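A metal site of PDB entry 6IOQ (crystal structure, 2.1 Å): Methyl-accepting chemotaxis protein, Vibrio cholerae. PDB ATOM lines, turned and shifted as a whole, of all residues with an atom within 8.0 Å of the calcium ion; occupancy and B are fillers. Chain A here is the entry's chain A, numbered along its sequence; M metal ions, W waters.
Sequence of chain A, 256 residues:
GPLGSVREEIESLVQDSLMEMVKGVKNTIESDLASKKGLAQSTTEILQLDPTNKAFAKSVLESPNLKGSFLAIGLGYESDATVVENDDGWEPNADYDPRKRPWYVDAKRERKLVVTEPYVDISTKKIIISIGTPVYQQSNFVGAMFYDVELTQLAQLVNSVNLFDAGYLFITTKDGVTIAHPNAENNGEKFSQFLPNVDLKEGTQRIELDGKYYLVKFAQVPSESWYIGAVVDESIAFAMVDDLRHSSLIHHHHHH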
ATOM      1  N   LYS A  58      15.721   8.974   6.233  1.00  0.00           N
ATOM      2  CA  LYS A  58      15.920   9.609   7.521  1.00  0.00           C
ATOM      3  C   LYS A  58      15.347  11.018   7.500  1.00  0.00           C
ATOM      4  O   LYS A  58      14.785  11.473   8.479  1.00  0.00           O
ATOM      5  CB  LYS A  58      17.386   9.673   7.909  1.00  0.00           C
ATOM      6  CG  LYS A  58      17.531  10.171   9.337  1.00  0.00           C
ATOM      7  CD  LYS A  58      18.952  10.387   9.780  1.00  0.00           C
ATOM      8  CE  LYS A  58      18.966  10.908  11.226  1.00  0.00           C
ATOM      9  NZ  LYS A  58      18.160  10.010  12.104  1.00  0.00           N
ATOM     10  N   GLU A  62      12.447  12.548   9.974  1.00  0.00           N
ATOM     11  CA  GLU A  62      12.818  13.654  10.834  1.00  0.00           C
ATOM     12  C   GLU A  62      12.025  14.924  10.567  1.00  0.00           C
ATOM     13  O   GLU A  62      12.149  15.888  11.324  1.00  0.00           O
ATOM     14  CB  GLU A  62      14.319  13.974  10.716  1.00  0.00           C
ATOM     15  CG  GLU A  62      15.242  12.832  11.180  1.00  0.00           C
ATOM     16  CD  GLU A  62      15.176  12.575  12.688  1.00  0.00           C
ATOM     17  OE1 GLU A  62      14.513  13.340  13.410  1.00  0.00           O
ATOM     18  OE2 GLU A  62      15.790  11.582  13.149  1.00  0.00           O
ATOM     19  N   ILE A  73       9.260   6.666  14.724  1.00  0.00           N
ATOM     20  CA  ILE A  73       9.073   6.067  13.418  1.00  0.00           C
ATOM     21  C   ILE A  73      10.372   5.462  12.938  1.00  0.00           C
ATOM     22  O   ILE A  73      11.457   6.017  13.147  1.00  0.00           O
ATOM     23  CB  ILE A  73       8.598   7.093  12.379  1.00  0.00           C
ATOM     24  CG1 ILE A  73       7.379   7.838  12.906  1.00  0.00           C
ATOM     25  CG2 ILE A  73       8.256   6.424  11.056  1.00  0.00           C
ATOM     26  CD1 ILE A  73       7.022   9.044  12.044  1.00  0.00           C
ATOM     27  N   VAL A  83      18.394  -0.471  10.307  1.00  0.00           N
ATOM     28  CA  VAL A  83      17.208   0.274  10.662  1.00  0.00           C
ATOM     29  C   VAL A  83      17.477   1.777  10.671  1.00  0.00           C
ATOM     30  O   VAL A  83      18.465   2.239  11.231  1.00  0.00           O
ATOM     31  CB  VAL A  83      16.649  -0.172  12.039  1.00  0.00           C
ATOM     32  CG1 VAL A  83      17.734  -0.182  13.093  1.00  0.00           C
ATOM     33  CG2 VAL A  83      15.516   0.736  12.491  1.00  0.00           C
ATOM     34  N   VAL A  84      16.603   2.541  10.016  1.00  0.00           N
ATOM     35  CA  VAL A  84      16.600   4.007  10.121  1.00  0.00           C
ATOM     36  C   VAL A  84      15.460   4.404  11.055  1.00  0.00           C
ATOM     37  O   VAL A  84      14.351   3.897  10.919  1.00  0.00           O
ATOM     38  CB  VAL A  84      16.410   4.683   8.740  1.00  0.00           C
ATOM     39  CG1 VAL A  84      16.416   6.203   8.875  1.00  0.00           C
ATOM     40  CG2 VAL A  84      17.488   4.247   7.766  1.00  0.00           C
ATOM     41  N   GLU A  85      15.714   5.272  12.016  1.00  0.00           N
ATOM     42  CA  GLU A  85      14.649   5.667  12.938  1.00  0.00           C
ATOM     43  C   GLU A  85      14.852   7.094  13.399  1.00  0.00           C
ATOM     44  O   GLU A  85      15.941   7.659  13.245  1.00  0.00           O
ATOM     45  CB  GLU A  85      14.599   4.695  14.121  1.00  0.00           C
ATOM     46  CG  GLU A  85      15.950   4.213  14.604  1.00  0.00           C
ATOM     47  CD  GLU A  85      16.689   5.261  15.444  1.00  0.00           C
ATOM     48  OE1 GLU A  85      16.011   6.099  16.068  1.00  0.00           O
ATOM     49  OE2 GLU A  85      17.935   5.250  15.475  1.00  0.00           O
ATOM     50  N   ASN A  86      13.806   7.682  13.976  1.00  0.00           N
ATOM     51  CA  ASN A  86      13.874   9.075  14.395  1.00  0.00           C
ATOM     52  C   ASN A  86      13.812   9.216  15.918  1.00  0.00           C
ATOM     53  O   ASN A  86      13.447  10.267  16.432  1.00  0.00           O
ATOM     54  CB  ASN A  86      12.749   9.901  13.738  1.00  0.00           C
ATOM     55  CG  ASN A  86      11.370   9.467  14.195  1.00  0.00           C
ATOM     56  OD1 ASN A  86      11.236   8.610  15.078  1.00  0.00           O
ATOM     57  ND2 ASN A  86      10.334  10.069  13.625  1.00  0.00           N
ATOM     58  N   ASP A  87      14.136   8.146  16.632  1.00  0.00           N
ATOM     59  CA  ASP A  87      14.161   8.204  18.089  1.00  0.00           C
ATOM     60  C   ASP A  87      15.474   8.849  18.556  1.00  0.00           C
ATOM     61  O   ASP A  87      16.551   8.298  18.340  1.00  0.00           O
ATOM     62  CB  ASP A  87      13.979   6.823  18.692  1.00  0.00           C
ATOM     63  CG  ASP A  87      13.674   6.857  20.173  1.00  0.00           C
ATOM     64  OD1 ASP A  87      14.187   7.759  20.869  1.00  0.00           O
ATOM     65  OD2 ASP A  87      12.908   5.994  20.650  1.00  0.00           O
ATOM     66  N   ASP A  88      15.361  10.022  19.162  1.00  0.00           N
ATOM     67  CA  ASP A  88      16.532  10.782  19.592  1.00  0.00           C
ATOM     68  C   ASP A  88      17.310  10.033  20.668  1.00  0.00           C
ATOM     69  O   ASP A  88      18.526  10.058  20.670  1.00  0.00           O
ATOM     70  CB  ASP A  88      16.131  12.156  20.114  1.00  0.00           C
ATOM     71  CG  ASP A  88      15.607  13.071  19.021  1.00  0.00           C
ATOM     72  OD1 ASP A  88      15.974  12.862  17.843  1.00  0.00           O
ATOM     73  OD2 ASP A  88      14.841  14.006  19.340  1.00  0.00           O
ATOM     74  N   GLY A  89      16.595   9.348  21.552  1.00  0.00           N
ATOM     75  CA  GLY A  89      17.209   8.737  22.703  1.00  0.00           C
ATOM     76  C   GLY A  89      17.389   7.235  22.596  1.00  0.00           C
ATOM     77  O   GLY A  89      17.368   6.533  23.597  1.00  0.00           O
ATOM     78  N   TRP A  90      17.542   6.743  21.371  1.00  0.00           N
ATOM     79  CA  TRP A  90      17.706   5.315  21.166  1.00  0.00           C
ATOM     80  C   TRP A  90      18.450   5.003  19.892  1.00  0.00           C
ATOM     81  O   TRP A  90      18.143   5.545  18.831  1.00  0.00           O
ATOM     82  CB  TRP A  90      16.352   4.609  21.152  1.00  0.00           C
ATOM     83  CG  TRP A  90      16.467   3.144  20.888  1.00  0.00           C
ATOM     84  CD1 TRP A  90      16.952   2.192  21.738  1.00  0.00           C
ATOM     85  CD2 TRP A  90      16.078   2.447  19.696  1.00  0.00           C
ATOM     86  NE1 TRP A  90      16.901   0.949  21.157  1.00  0.00           N
ATOM     87  CE2 TRP A  90      16.369   1.078  19.888  1.00  0.00           C
ATOM     88  CE3 TRP A  90      15.521   2.854  18.473  1.00  0.00           C
ATOM     89  CZ2 TRP A  90      16.111   0.106  18.924  1.00  0.00           C
ATOM     90  CZ3 TRP A  90      15.271   1.882  17.503  1.00  0.00           C
ATOM     91  CH2 TRP A  90      15.567   0.532  17.738  1.00  0.00           C
ATOM     92  N   GLU A  91      19.442   4.138  20.013  1.00  0.00           N
ATOM     93  CA  GLU A  91      20.174   3.581  18.894  1.00  0.00           C
ATOM     94  C   GLU A  91      20.133   2.062  19.072  1.00  0.00           C
ATOM     95  O   GLU A  91      20.360   1.556  20.174  1.00  0.00           O
ATOM     96  CB  GLU A  91      21.612   4.114  18.857  1.00  0.00           C
ATOM     97  CG  GLU A  91      22.445   3.711  17.651  1.00  0.00           C
ATOM     98  CD  GLU A  91      22.089   4.485  16.378  1.00  0.00           C
ATOM     99  OE1 GLU A  91      21.127   5.282  16.398  1.00  0.00           O
ATOM    100  OE2 GLU A  91      22.778   4.282  15.349  1.00  0.00           O
ATOM    101  N   PRO A  92      19.820   1.314  17.998  1.00  0.00           N
ATOM    102  CA  PRO A  92      19.653  -0.145  18.093  1.00  0.00           C
ATOM    103  C   PRO A  92      20.931  -0.899  18.469  1.00  0.00           C
ATOM    104  O   PRO A  92      22.001  -0.577  17.960  1.00  0.00           O
ATOM    105  CB  PRO A  92      19.210  -0.522  16.679  1.00  0.00           C
ATOM    106  CG  PRO A  92      19.748   0.561  15.824  1.00  0.00           C
ATOM    107  CD  PRO A  92      19.593   1.810  16.640  1.00  0.00           C
ATOM    108  N   SER A 123      12.733   0.650  22.860  1.00  0.00           N
ATOM    109  CA  SER A 123      13.251   1.972  23.240  1.00  0.00           C
ATOM    110  C   SER A 123      12.798   2.441  24.609  1.00  0.00           C
ATOM    111  O   SER A 123      13.617   2.707  25.484  1.00  0.00           O
ATOM    112  CB  SER A 123      12.834   3.020  22.198  1.00  0.00           C
ATOM    113  OG  SER A 123      13.247   4.325  22.600  1.00  0.00           O
HETATM  114 CA    CA M   1      18.126   7.023  17.199  1.00  0.00          CA
HETATM  115  O   HOH W   1      17.568   8.546  15.428  1.00  0.00           O
HETATM  116  O   HOH W   2      19.590   8.513  18.229  1.00  0.00           O
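The backbone NH (N) of Gly 89 lies within hydrogen-bond range of the side-chain carboxylate (OD1) of Asp 87. The side-chain carboxylate (OD2) of Asp 87 lies within hydrogen-bond range of the side-chain hydroxyl (OG) of Ser 123. The backbone carbonyl oxygen of Glu 85 lies within hydrogen-bond range of the side-chain amino group of Lys 58 (3.4 Å).
OE1 of Glu 91 touches the calcium ion, at 3.6 Å. Within 4 Å of the calcium ion: Glu 85, Asp 87, Trp 90 and Glu 91. Along chain A the residues within 4 Å of the calcium ion span positions 85 to 91. The nearest printed residue that does not touch the calcium ion is Asp 88 (4.5 Å).
The calcium ion is bound by the backbone carbonyl oxygen (O) of Trp 90 (2.2 Å), the backbone carbonyl oxygen (O) of Asp 87 (2.3 Å), water W2 (2.3 Å), water W1 (2.4 Å), the side-chain carboxylate (OE2) of Glu 85 (2.5 Å) and the side-chain carboxylate (OE1) of Glu 85 (2.6 Å).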
